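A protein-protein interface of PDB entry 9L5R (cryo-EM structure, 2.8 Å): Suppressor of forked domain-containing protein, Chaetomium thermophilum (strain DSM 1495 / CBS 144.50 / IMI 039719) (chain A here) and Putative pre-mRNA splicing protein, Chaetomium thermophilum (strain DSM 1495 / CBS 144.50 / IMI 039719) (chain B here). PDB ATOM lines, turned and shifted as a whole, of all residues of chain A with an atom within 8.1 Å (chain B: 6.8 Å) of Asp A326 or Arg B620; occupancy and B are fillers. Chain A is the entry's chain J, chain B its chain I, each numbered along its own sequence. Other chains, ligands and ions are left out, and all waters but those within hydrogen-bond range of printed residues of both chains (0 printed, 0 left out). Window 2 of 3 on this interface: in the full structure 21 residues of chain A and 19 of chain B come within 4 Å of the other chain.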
ATOM      1  N   TYR A 314     -13.082 -11.582 -10.002  1.00  0.00           N
ATOM      2  CA  TYR A 314     -12.024 -12.137  -9.169  1.00  0.00           C
ATOM      3  C   TYR A 314     -11.811 -13.614  -9.457  1.00  0.00           C
ATOM      4  O   TYR A 314     -10.681 -14.097  -9.366  1.00  0.00           O
ATOM      5  CB  TYR A 314     -12.351 -11.952  -7.696  1.00  0.00           C
ATOM      6  CG  TYR A 314     -12.238 -10.549  -7.154  1.00  0.00           C
ATOM      7  CD1 TYR A 314     -11.207  -9.707  -7.534  1.00  0.00           C
ATOM      8  CD2 TYR A 314     -13.162 -10.076  -6.236  1.00  0.00           C
ATOM      9  CE1 TYR A 314     -11.112  -8.425  -7.025  1.00  0.00           C
ATOM     10  CE2 TYR A 314     -13.076  -8.804  -5.726  1.00  0.00           C
ATOM     11  CZ  TYR A 314     -12.051  -7.983  -6.122  1.00  0.00           C
ATOM     12  OH  TYR A 314     -11.961  -6.711  -5.614  1.00  0.00           O
ATOM     13  N   GLN A 317      -9.622 -13.712 -12.370  1.00  0.00           N
ATOM     14  CA  GLN A 317      -8.266 -13.323 -11.994  1.00  0.00           C
ATOM     15  C   GLN A 317      -7.539 -14.456 -11.275  1.00  0.00           C
ATOM     16  O   GLN A 317      -6.342 -14.668 -11.496  1.00  0.00           O
ATOM     17  CB  GLN A 317      -8.303 -12.062 -11.132  1.00  0.00           C
ATOM     18  CG  GLN A 317      -8.499 -10.788 -11.939  1.00  0.00           C
ATOM     19  CD  GLN A 317      -8.805  -9.583 -11.077  1.00  0.00           C
ATOM     20  OE1 GLN A 317      -9.093  -9.714  -9.891  1.00  0.00           O
ATOM     21  NE2 GLN A 317      -8.742  -8.397 -11.672  1.00  0.00           N
ATOM     22  N   ASN A 321      -4.117 -16.265 -12.413  1.00  0.00           N
ATOM     23  CA  ASN A 321      -3.035 -16.342 -11.432  1.00  0.00           C
ATOM     24  C   ASN A 321      -3.580 -16.916 -10.134  1.00  0.00           C
ATOM     25  O   ASN A 321      -4.256 -16.202  -9.372  1.00  0.00           O
ATOM     26  CB  ASN A 321      -2.425 -14.965 -11.193  1.00  0.00           C
ATOM     27  CG  ASN A 321      -1.747 -14.414 -12.427  1.00  0.00           C
ATOM     28  OD1 ASN A 321      -0.843 -15.035 -12.982  1.00  0.00           O
ATOM     29  ND2 ASN A 321      -2.188 -13.244 -12.870  1.00  0.00           N
ATOM     30  N   LYS A 323      -2.031 -17.598  -7.475  1.00  0.00           N
ATOM     31  CA  LYS A 323      -1.208 -17.210  -6.340  1.00  0.00           C
ATOM     32  C   LYS A 323      -1.197 -15.708  -6.083  1.00  0.00           C
ATOM     33  O   LYS A 323      -0.347 -15.228  -5.327  1.00  0.00           O
ATOM     34  CB  LYS A 323       0.216 -17.724  -6.552  1.00  0.00           C
ATOM     35  CG  LYS A 323       0.900 -17.095  -7.750  1.00  0.00           C
ATOM     36  CD  LYS A 323       2.284 -17.669  -7.970  1.00  0.00           C
ATOM     37  CE  LYS A 323       2.951 -17.003  -9.159  1.00  0.00           C
ATOM     38  NZ  LYS A 323       2.262 -17.345 -10.433  1.00  0.00           N
ATOM     39  N   ASN A 324      -2.114 -14.951  -6.682  1.00  0.00           N
ATOM     40  CA  ASN A 324      -2.174 -13.510  -6.436  1.00  0.00           C
ATOM     41  C   ASN A 324      -2.845 -13.273  -5.089  1.00  0.00           C
ATOM     42  O   ASN A 324      -4.067 -13.369  -4.936  1.00  0.00           O
ATOM     43  CB  ASN A 324      -2.889 -12.786  -7.566  1.00  0.00           C
ATOM     44  CG  ASN A 324      -2.285 -11.427  -7.845  1.00  0.00           C
ATOM     45  OD1 ASN A 324      -1.322 -11.025  -7.195  1.00  0.00           O
ATOM     46  ND2 ASN A 324      -2.829 -10.722  -8.828  1.00  0.00           N
ATOM     47  N   TYR A 325      -2.016 -12.950  -4.097  1.00  0.00           N
ATOM     48  CA  TYR A 325      -2.470 -12.951  -2.713  1.00  0.00           C
ATOM     49  C   TYR A 325      -3.358 -11.751  -2.408  1.00  0.00           C
ATOM     50  O   TYR A 325      -4.332 -11.874  -1.661  1.00  0.00           O
ATOM     51  CB  TYR A 325      -1.262 -13.008  -1.782  1.00  0.00           C
ATOM     52  CG  TYR A 325      -0.728 -14.416  -1.637  1.00  0.00           C
ATOM     53  CD1 TYR A 325      -1.399 -15.364  -0.878  1.00  0.00           C
ATOM     54  CD2 TYR A 325       0.433 -14.805  -2.294  1.00  0.00           C
ATOM     55  CE1 TYR A 325      -0.916 -16.657  -0.759  1.00  0.00           C
ATOM     56  CE2 TYR A 325       0.922 -16.093  -2.183  1.00  0.00           C
ATOM     57  CZ  TYR A 325       0.245 -17.013  -1.414  1.00  0.00           C
ATOM     58  OH  TYR A 325       0.729 -18.295  -1.302  1.00  0.00           O
ATOM     59  N   ASP A 326      -3.029 -10.576  -2.951  1.00  0.00           N
ATOM     60  CA  ASP A 326      -3.899  -9.418  -2.763  1.00  0.00           C
ATOM     61  C   ASP A 326      -5.245  -9.590  -3.462  1.00  0.00           C
ATOM     62  O   ASP A 326      -6.271  -9.118  -2.955  1.00  0.00           O
ATOM     63  CB  ASP A 326      -3.178  -8.144  -3.215  1.00  0.00           C
ATOM     64  CG  ASP A 326      -2.754  -8.182  -4.674  1.00  0.00           C
ATOM     65  OD1 ASP A 326      -2.948  -9.217  -5.346  1.00  0.00           O
ATOM     66  OD2 ASP A 326      -2.217  -7.159  -5.152  1.00  0.00           O
ATOM     67  N   VAL A 327      -5.260 -10.272  -4.610  1.00  0.00           N
ATOM     68  CA  VAL A 327      -6.519 -10.640  -5.261  1.00  0.00           C
ATOM     69  C   VAL A 327      -7.320 -11.575  -4.362  1.00  0.00           C
ATOM     70  O   VAL A 327      -8.543 -11.432  -4.208  1.00  0.00           O
ATOM     71  CB  VAL A 327      -6.238 -11.265  -6.639  1.00  0.00           C
ATOM     72  CG1 VAL A 327      -7.408 -12.103  -7.124  1.00  0.00           C
ATOM     73  CG2 VAL A 327      -5.927 -10.172  -7.646  1.00  0.00           C
ATOM     74  N   TRP A 328      -6.629 -12.534  -3.737  1.00  0.00           N
ATOM     75  CA  TRP A 328      -7.279 -13.442  -2.797  1.00  0.00           C
ATOM     76  C   TRP A 328      -7.851 -12.689  -1.601  1.00  0.00           C
ATOM     77  O   TRP A 328      -8.951 -12.993  -1.137  1.00  0.00           O
ATOM     78  CB  TRP A 328      -6.281 -14.499  -2.332  1.00  0.00           C
ATOM     79  CG  TRP A 328      -6.269 -15.728  -3.180  1.00  0.00           C
ATOM     80  CD1 TRP A 328      -5.262 -16.145  -3.998  1.00  0.00           C
ATOM     81  CD2 TRP A 328      -7.311 -16.701  -3.299  1.00  0.00           C
ATOM     82  NE1 TRP A 328      -5.611 -17.319  -4.617  1.00  0.00           N
ATOM     83  CE2 TRP A 328      -6.866 -17.680  -4.205  1.00  0.00           C
ATOM     84  CE3 TRP A 328      -8.578 -16.838  -2.725  1.00  0.00           C
ATOM     85  CZ2 TRP A 328      -7.639 -18.783  -4.548  1.00  0.00           C
ATOM     86  CZ3 TRP A 328      -9.344 -17.932  -3.069  1.00  0.00           C
ATOM     87  CH2 TRP A 328      -8.874 -18.890  -3.974  1.00  0.00           C
ATOM     88  N   PHE A 329      -7.119 -11.689  -1.107  1.00  0.00           N
ATOM     89  CA  PHE A 329      -7.573 -10.863   0.011  1.00  0.00           C
ATOM     90  C   PHE A 329      -8.791 -10.022  -0.348  1.00  0.00           C
ATOM     91  O   PHE A 329      -9.711  -9.887   0.467  1.00  0.00           O
ATOM     92  CB  PHE A 329      -6.448  -9.927   0.464  1.00  0.00           C
ATOM     93  CG  PHE A 329      -5.274 -10.624   1.106  1.00  0.00           C
ATOM     94  CD1 PHE A 329      -5.362 -11.939   1.533  1.00  0.00           C
ATOM     95  CD2 PHE A 329      -4.071  -9.957   1.269  1.00  0.00           C
ATOM     96  CE1 PHE A 329      -4.279 -12.567   2.111  1.00  0.00           C
ATOM     97  CE2 PHE A 329      -2.987 -10.584   1.849  1.00  0.00           C
ATOM     98  CZ  PHE A 329      -3.094 -11.890   2.268  1.00  0.00           C
ATOM     99  N   ASP A 330      -8.812  -9.441  -1.544  1.00  0.00           N
ATOM    100  CA  ASP A 330      -9.960  -8.664  -1.988  1.00  0.00           C
ATOM    101  C   ASP A 330     -11.199  -9.512  -2.225  1.00  0.00           C
ATOM    102  O   ASP A 330     -12.296  -9.098  -1.838  1.00  0.00           O
ATOM    103  CB  ASP A 330      -9.617  -7.905  -3.268  1.00  0.00           C
ATOM    104  CG  ASP A 330      -8.998  -6.561  -2.986  1.00  0.00           C
ATOM    105  OD1 ASP A 330      -9.455  -5.883  -2.043  1.00  0.00           O
ATOM    106  OD2 ASP A 330      -8.058  -6.182  -3.707  1.00  0.00           O
ATOM    107  N   PHE A 331     -11.045 -10.685  -2.839  1.00  0.00           N
ATOM    108  CA  PHE A 331     -12.170 -11.602  -2.991  1.00  0.00           C
ATOM    109  C   PHE A 331     -12.613 -12.167  -1.650  1.00  0.00           C
ATOM    110  O   PHE A 331     -13.804 -12.437  -1.444  1.00  0.00           O
ATOM    111  CB  PHE A 331     -11.785 -12.682  -3.995  1.00  0.00           C
ATOM    112  CG  PHE A 331     -12.851 -13.684  -4.270  1.00  0.00           C
ATOM    113  CD1 PHE A 331     -13.950 -13.372  -5.046  1.00  0.00           C
ATOM    114  CD2 PHE A 331     -12.664 -14.992  -3.901  1.00  0.00           C
ATOM    115  CE1 PHE A 331     -14.901 -14.323  -5.339  1.00  0.00           C
ATOM    116  CE2 PHE A 331     -13.595 -15.943  -4.213  1.00  0.00           C
ATOM    117  CZ  PHE A 331     -14.720 -15.611  -4.922  1.00  0.00           C
ATOM    118  N   ALA A 332     -11.677 -12.293  -0.710  1.00  0.00           N
ATOM    119  CA  ALA A 332     -12.004 -12.628   0.666  1.00  0.00           C
ATOM    120  C   ALA A 332     -12.924 -11.588   1.283  1.00  0.00           C
ATOM    121  O   ALA A 332     -13.982 -11.921   1.824  1.00  0.00           O
ATOM    122  CB  ALA A 332     -10.714 -12.726   1.467  1.00  0.00           C
ATOM    123  N   ARG A 333     -12.530 -10.315   1.199  1.00  0.00           N
ATOM    124  CA  ARG A 333     -13.345  -9.247   1.767  1.00  0.00           C
ATOM    125  C   ARG A 333     -14.679  -9.121   1.050  1.00  0.00           C
ATOM    126  O   ARG A 333     -15.691  -8.796   1.680  1.00  0.00           O
ATOM    127  CB  ARG A 333     -12.599  -7.918   1.715  1.00  0.00           C
ATOM    128  CG  ARG A 333     -11.445  -7.817   2.685  1.00  0.00           C
ATOM    129  CD  ARG A 333     -11.919  -7.820   4.129  1.00  0.00           C
ATOM    130  NE  ARG A 333     -12.776  -6.684   4.447  1.00  0.00           N
ATOM    131  CZ  ARG A 333     -13.500  -6.581   5.554  1.00  0.00           C
ATOM    132  NH1 ARG A 333     -13.473  -7.518   6.487  1.00  0.00           N
ATOM    133  NH2 ARG A 333     -14.263  -5.506   5.732  1.00  0.00           N
ATOM    134  N   ARG A 366       2.476 -13.042   3.554  1.00  0.00           N
ATOM    135  CA  ARG A 366       1.113 -12.931   3.072  1.00  0.00           C
ATOM    136  C   ARG A 366       0.340 -14.235   3.203  1.00  0.00           C
ATOM    137  O   ARG A 366      -0.860 -14.199   3.482  1.00  0.00           O
ATOM    138  CB  ARG A 366       1.118 -12.436   1.625  1.00  0.00           C
ATOM    139  CG  ARG A 366       1.337 -10.932   1.543  1.00  0.00           C
ATOM    140  CD  ARG A 366       1.152 -10.356   0.153  1.00  0.00           C
ATOM    141  NE  ARG A 366       1.004  -8.906   0.213  1.00  0.00           N
ATOM    142  CZ  ARG A 366       1.633  -8.048  -0.579  1.00  0.00           C
ATOM    143  NH1 ARG A 366       2.471  -8.459  -1.517  1.00  0.00           N
ATOM    144  NH2 ARG A 366       1.420  -6.745  -0.422  1.00  0.00           N
ATOM    145  N   LEU A 370      -2.921 -14.625   5.440  1.00  0.00           N
ATOM    146  CA  LEU A 370      -4.183 -15.181   4.968  1.00  0.00           C
ATOM    147  C   LEU A 370      -4.780 -16.148   5.985  1.00  0.00           C
ATOM    148  O   LEU A 370      -6.001 -16.159   6.206  1.00  0.00           O
ATOM    149  CB  LEU A 370      -3.944 -15.869   3.627  1.00  0.00           C
ATOM    150  CG  LEU A 370      -5.045 -16.551   2.829  1.00  0.00           C
ATOM    151  CD1 LEU A 370      -6.139 -15.574   2.452  1.00  0.00           C
ATOM    152  CD2 LEU A 370      -4.398 -17.147   1.593  1.00  0.00           C
ATOM    153  N   TYR B 602      -7.606   7.667 -13.665  1.00  0.00           N
ATOM    154  CA  TYR B 602      -6.666   6.680 -13.161  1.00  0.00           C
ATOM    155  C   TYR B 602      -5.957   7.178 -11.910  1.00  0.00           C
ATOM    156  O   TYR B 602      -5.674   6.389 -10.997  1.00  0.00           O
ATOM    157  CB  TYR B 602      -5.663   6.338 -14.247  1.00  0.00           C
ATOM    158  CG  TYR B 602      -6.039   5.165 -15.119  1.00  0.00           C
ATOM    159  CD1 TYR B 602      -5.959   3.870 -14.641  1.00  0.00           C
ATOM    160  CD2 TYR B 602      -6.448   5.354 -16.428  1.00  0.00           C
ATOM    161  CE1 TYR B 602      -6.287   2.800 -15.439  1.00  0.00           C
ATOM    162  CE2 TYR B 602      -6.779   4.294 -17.230  1.00  0.00           C
ATOM    163  CZ  TYR B 602      -6.698   3.019 -16.732  1.00  0.00           C
ATOM    164  OH  TYR B 602      -7.023   1.957 -17.537  1.00  0.00           O
ATOM    165  N   LEU B 614      -5.337  -1.743  -1.209  1.00  0.00           N
ATOM    166  CA  LEU B 614      -3.954  -2.174  -1.073  1.00  0.00           C
ATOM    167  C   LEU B 614      -3.061  -1.465  -2.086  1.00  0.00           C
ATOM    168  O   LEU B 614      -3.433  -1.229  -3.242  1.00  0.00           O
ATOM    169  CB  LEU B 614      -3.836  -3.694  -1.227  1.00  0.00           C
ATOM    170  CG  LEU B 614      -3.963  -4.530   0.050  1.00  0.00           C
ATOM    171  CD1 LEU B 614      -5.398  -4.633   0.530  1.00  0.00           C
ATOM    172  CD2 LEU B 614      -3.373  -5.910  -0.164  1.00  0.00           C
ATOM    173  N   ALA B 615      -1.853  -1.134  -1.629  1.00  0.00           N
ATOM    174  CA  ALA B 615      -0.911  -0.383  -2.446  1.00  0.00           C
ATOM    175  C   ALA B 615      -0.379  -1.177  -3.628  1.00  0.00           C
ATOM    176  O   ALA B 615      -0.004  -0.575  -4.635  1.00  0.00           O
ATOM    177  CB  ALA B 615       0.260   0.109  -1.594  1.00  0.00           C
ATOM    178  N   ARG B 616      -0.338  -2.509  -3.542  1.00  0.00           N
ATOM    179  CA  ARG B 616      -0.002  -3.307  -4.720  1.00  0.00           C
ATOM    180  C   ARG B 616      -1.051  -3.137  -5.814  1.00  0.00           C
ATOM    181  O   ARG B 616      -0.718  -3.006  -7.003  1.00  0.00           O
ATOM    182  CB  ARG B 616       0.135  -4.778  -4.334  1.00  0.00           C
ATOM    183  CG  ARG B 616       1.365  -5.093  -3.508  1.00  0.00           C
ATOM    184  CD  ARG B 616       2.595  -5.107  -4.393  1.00  0.00           C
ATOM    185  NE  ARG B 616       2.445  -6.048  -5.496  1.00  0.00           N
ATOM    186  CZ  ARG B 616       3.024  -5.915  -6.681  1.00  0.00           C
ATOM    187  NH1 ARG B 616       3.803  -4.881  -6.957  1.00  0.00           N
ATOM    188  NH2 ARG B 616       2.814  -6.838  -7.614  1.00  0.00           N
ATOM    189  N   HIS B 617      -2.325  -3.125  -5.424  1.00  0.00           N
ATOM    190  CA  HIS B 617      -3.397  -2.862  -6.372  1.00  0.00           C
ATOM    191  C   HIS B 617      -3.297  -1.452  -6.928  1.00  0.00           C
ATOM    192  O   HIS B 617      -3.537  -1.230  -8.121  1.00  0.00           O
ATOM    193  CB  HIS B 617      -4.745  -3.077  -5.695  1.00  0.00           C
ATOM    194  CG  HIS B 617      -5.149  -4.511  -5.601  1.00  0.00           C
ATOM    195  ND1 HIS B 617      -5.434  -5.279  -6.709  1.00  0.00           N
ATOM    196  CD2 HIS B 617      -5.292  -5.324  -4.531  1.00  0.00           C
ATOM    197  CE1 HIS B 617      -5.752  -6.501  -6.322  1.00  0.00           C
ATOM    198  NE2 HIS B 617      -5.677  -6.554  -5.006  1.00  0.00           N
ATOM    199  N   ALA B 618      -2.937  -0.489  -6.078  1.00  0.00           N
ATOM    200  CA  ALA B 618      -2.738   0.875  -6.559  1.00  0.00           C
ATOM    201  C   ALA B 618      -1.595   0.950  -7.565  1.00  0.00           C
ATOM    202  O   ALA B 618      -1.679   1.683  -8.555  1.00  0.00           O
ATOM    203  CB  ALA B 618      -2.481   1.813  -5.385  1.00  0.00           C
ATOM    204  N   MET B 619      -0.528   0.185  -7.336  1.00  0.00           N
ATOM    205  CA  MET B 619       0.593   0.165  -8.271  1.00  0.00           C
ATOM    206  C   MET B 619       0.200  -0.443  -9.611  1.00  0.00           C
ATOM    207  O   MET B 619       0.618   0.052 -10.664  1.00  0.00           O
ATOM    208  CB  MET B 619       1.777  -0.588  -7.669  1.00  0.00           C
ATOM    209  CG  MET B 619       2.502   0.160  -6.565  1.00  0.00           C
ATOM    210  SD  MET B 619       2.720   1.911  -6.930  1.00  0.00           S
ATOM    211  CE  MET B 619       1.684   2.657  -5.676  1.00  0.00           C
ATOM    212  N   ARG B 620      -0.595  -1.515  -9.604  1.00  0.00           N
ATOM    213  CA  ARG B 620      -1.007  -2.072 -10.893  1.00  0.00           C
ATOM    214  C   ARG B 620      -2.001  -1.153 -11.605  1.00  0.00           C
ATOM    215  O   ARG B 620      -2.009  -1.088 -12.844  1.00  0.00           O
ATOM    216  CB  ARG B 620      -1.565  -3.487 -10.718  1.00  0.00           C
ATOM    217  CG  ARG B 620      -2.996  -3.598 -10.239  1.00  0.00           C
ATOM    218  CD  ARG B 620      -3.408  -5.051 -10.088  1.00  0.00           C
ATOM    219  NE  ARG B 620      -2.869  -5.653  -8.876  1.00  0.00           N
ATOM    220  CZ  ARG B 620      -1.818  -6.459  -8.845  1.00  0.00           C
ATOM    221  NH1 ARG B 620      -1.156  -6.774  -9.947  1.00  0.00           N
ATOM    222  NH2 ARG B 620      -1.419  -6.961  -7.681  1.00  0.00           N
ATOM    223  N   ILE B 621      -2.798  -0.399 -10.840  1.00  0.00           N
ATOM    224  CA  ILE B 621      -3.657   0.625 -11.425  1.00  0.00           C
ATOM    225  C   ILE B 621      -2.815   1.703 -12.094  1.00  0.00           C
ATOM    226  O   ILE B 621      -3.108   2.134 -13.215  1.00  0.00           O
ATOM    227  CB  ILE B 621      -4.586   1.207 -10.343  1.00  0.00           C
ATOM    228  CG1 ILE B 621      -5.751   0.257 -10.087  1.00  0.00           C
ATOM    229  CG2 ILE B 621      -5.106   2.572 -10.730  1.00  0.00           C
ATOM    230  CD1 ILE B 621      -6.402   0.452  -8.753  1.00  0.00           C
ATOM    231  N   TYR B 622      -1.737   2.127 -11.433  1.00  0.00           N
ATOM    232  CA  TYR B 622      -0.848   3.124 -12.021  1.00  0.00           C
ATOM    233  C   TYR B 622      -0.097   2.582 -13.231  1.00  0.00           C
ATOM    234  O   TYR B 622       0.233   3.346 -14.139  1.00  0.00           O
ATOM    235  CB  TYR B 622       0.142   3.630 -10.980  1.00  0.00           C
ATOM    236  CG  TYR B 622      -0.464   4.537  -9.941  1.00  0.00           C
ATOM    237  CD1 TYR B 622      -1.337   5.546 -10.300  1.00  0.00           C
ATOM    238  CD2 TYR B 622      -0.150   4.391  -8.603  1.00  0.00           C
ATOM    239  CE1 TYR B 622      -1.890   6.376  -9.353  1.00  0.00           C
ATOM    240  CE2 TYR B 622      -0.701   5.210  -7.649  1.00  0.00           C
ATOM    241  CZ  TYR B 622      -1.569   6.203  -8.029  1.00  0.00           C
ATOM    242  OH  TYR B 622      -2.117   7.027  -7.075  1.00  0.00           O
ATOM    243  N   GLU B 623       0.187   1.280 -13.265  1.00  0.00           N
ATOM    244  CA  GLU B 623       0.817   0.700 -14.449  1.00  0.00           C
ATOM    245  C   GLU B 623      -0.126   0.717 -15.648  1.00  0.00           C
ATOM    246  O   GLU B 623       0.272   1.099 -16.761  1.00  0.00           O
ATOM    247  CB  GLU B 623       1.279  -0.723 -14.154  1.00  0.00           C
ATOM    248  CG  GLU B 623       2.395  -1.198 -15.056  1.00  0.00           C
ATOM    249  CD  GLU B 623       1.893  -2.010 -16.229  1.00  0.00           C
ATOM    250  OE1 GLU B 623       0.984  -2.840 -16.031  1.00  0.00           O
ATOM    251  OE2 GLU B 623       2.403  -1.812 -17.351  1.00  0.00           O
ATOM    252  N   ARG B 624      -1.385   0.319 -15.434  1.00  0.00           N
ATOM    253  CA  ARG B 624      -2.392   0.470 -16.482  1.00  0.00           C
ATOM    254  C   ARG B 624      -2.558   1.928 -16.893  1.00  0.00           C
ATOM    255  O   ARG B 624      -2.790   2.221 -18.070  1.00  0.00           O
ATOM    256  CB  ARG B 624      -3.734  -0.089 -16.017  1.00  0.00           C
ATOM    257  CG  ARG B 624      -3.768  -1.589 -15.846  1.00  0.00           C
ATOM    258  CD  ARG B 624      -4.818  -1.987 -14.831  1.00  0.00           C
ATOM    259  NE  ARG B 624      -6.165  -1.828 -15.359  1.00  0.00           N
ATOM    260  CZ  ARG B 624      -7.118  -1.114 -14.776  1.00  0.00           C
ATOM    261  NH1 ARG B 624      -6.907  -0.485 -13.634  1.00  0.00           N
ATOM    262  NH2 ARG B 624      -8.312  -1.031 -15.353  1.00  0.00           N
ATOM    263  N   ALA B 625      -2.427   2.848 -15.937  1.00  0.00           N
ATOM    264  CA  ALA B 625      -2.494   4.273 -16.235  1.00  0.00           C
ATOM    265  C   ALA B 625      -1.365   4.705 -17.154  1.00  0.00           C
ATOM    266  O   ALA B 625      -1.584   5.452 -18.112  1.00  0.00           O
ATOM    267  CB  ALA B 625      -2.442   5.067 -14.940  1.00  0.00           C
ATOM    268  N   ARG B 627       0.153   2.883 -19.229  1.00  0.00           N
ATOM    269  CA  ARG B 627      -0.148   2.381 -20.565  1.00  0.00           C
ATOM    270  C   ARG B 627      -1.240   3.194 -21.258  1.00  0.00           C
ATOM    271  O   ARG B 627      -1.189   3.369 -22.480  1.00  0.00           O
ATOM    272  CB  ARG B 627      -0.541   0.908 -20.499  1.00  0.00           C
ATOM    273  CG  ARG B 627       0.641  -0.025 -20.334  1.00  0.00           C
ATOM    274  CD  ARG B 627       0.294  -1.446 -20.730  1.00  0.00           C
ATOM    275  NE  ARG B 627      -0.172  -2.225 -19.591  1.00  0.00           N
ATOM    276  CZ  ARG B 627      -1.448  -2.448 -19.306  1.00  0.00           C
ATOM    277  NH1 ARG B 627      -2.419  -1.966 -20.065  1.00  0.00           N
ATOM    278  NH2 ARG B 627      -1.758  -3.174 -18.238  1.00  0.00           N
ATOM    279  N   TYR B 641       4.084   7.478 -11.269  1.00  0.00           N
ATOM    280  CA  TYR B 641       4.195   6.075 -10.886  1.00  0.00           C
ATOM    281  C   TYR B 641       5.502   5.814 -10.155  1.00  0.00           C
ATOM    282  O   TYR B 641       5.520   5.121  -9.136  1.00  0.00           O
ATOM    283  CB  TYR B 641       4.087   5.204 -12.139  1.00  0.00           C
ATOM    284  CG  TYR B 641       4.008   3.703 -11.932  1.00  0.00           C
ATOM    285  CD1 TYR B 641       3.650   3.150 -10.709  1.00  0.00           C
ATOM    286  CD2 TYR B 641       4.275   2.840 -12.983  1.00  0.00           C
ATOM    287  CE1 TYR B 641       3.579   1.782 -10.539  1.00  0.00           C
ATOM    288  CE2 TYR B 641       4.211   1.476 -12.822  1.00  0.00           C
ATOM    289  CZ  TYR B 641       3.860   0.951 -11.601  1.00  0.00           C
ATOM    290  OH  TYR B 641       3.791  -0.413 -11.447  1.00  0.00           O
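Of the 15 printed residues of chain B, 4 touch a printed residue of chain A. Printed residues of chain B that touch a printed residue of chain A: Leu B614, Arg B616, His B617 and Arg B620. Hydrophobic or aromatic side chains of chain B that line the printed part of chain A: Leu B614 and His B617. Of the 16 printed residues of chain A, 4 touch a printed residue of chain B. Among the printed residues, Asp or Glu carboxylates within 4 Å of a Lys or Arg side-chain nitrogen of the other chain: Asp A326 with Arg B620 (2.7 Å).
A ring nitrogen (ND1) of His B617 sits at hydrogen-bond distance from the guanidinium group (NE) of Arg B620 (3.4 Å). OD1 of Asn A324 lies close to OD1 of Asp A326, 3.1 Å away.
O of Asp A326 lies within hydrogen-bond range of NE2 of His B617 (3.3 Å). The side-chain carboxylate of Asp A330 is in hydrogen-bond range of a ring nitrogen (NE2) of His B617 (2.7 Å). The side-chain carboxylate (OD2) of Asp A326 is in salt-bridge range of the guanidinium group (NH2) of Arg B620 (2.7 Å).
Of chain B, only Leu B614, Arg B616, His B617 and Arg B620 come within 4 Å of Asp A326. Printed residues of chain B within 4 Å of Val A327: His B617. Printed residues of chain B within 4 Å of Asp A330: His B617 (2.7 Å). Printed residues of chain A within 4 Å of Arg B616: Asp A326 and Arg A366. Ala B625 touches none of the printed residues of chain A. Arg B627 touches none of the printed residues of chain A. The nearest residue of chain B that does not touch Asp A326 is Ala B615 (6.4 Å).
Among the printed residues, merely in contact across the chains: Asp A326 with Leu B614 (3.8 Å), Asp A326 with Arg B616 (3.4 Å), Val A327 with His B617 (3.8 Å) and Arg A366 with Arg B616 (3.5 Å).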
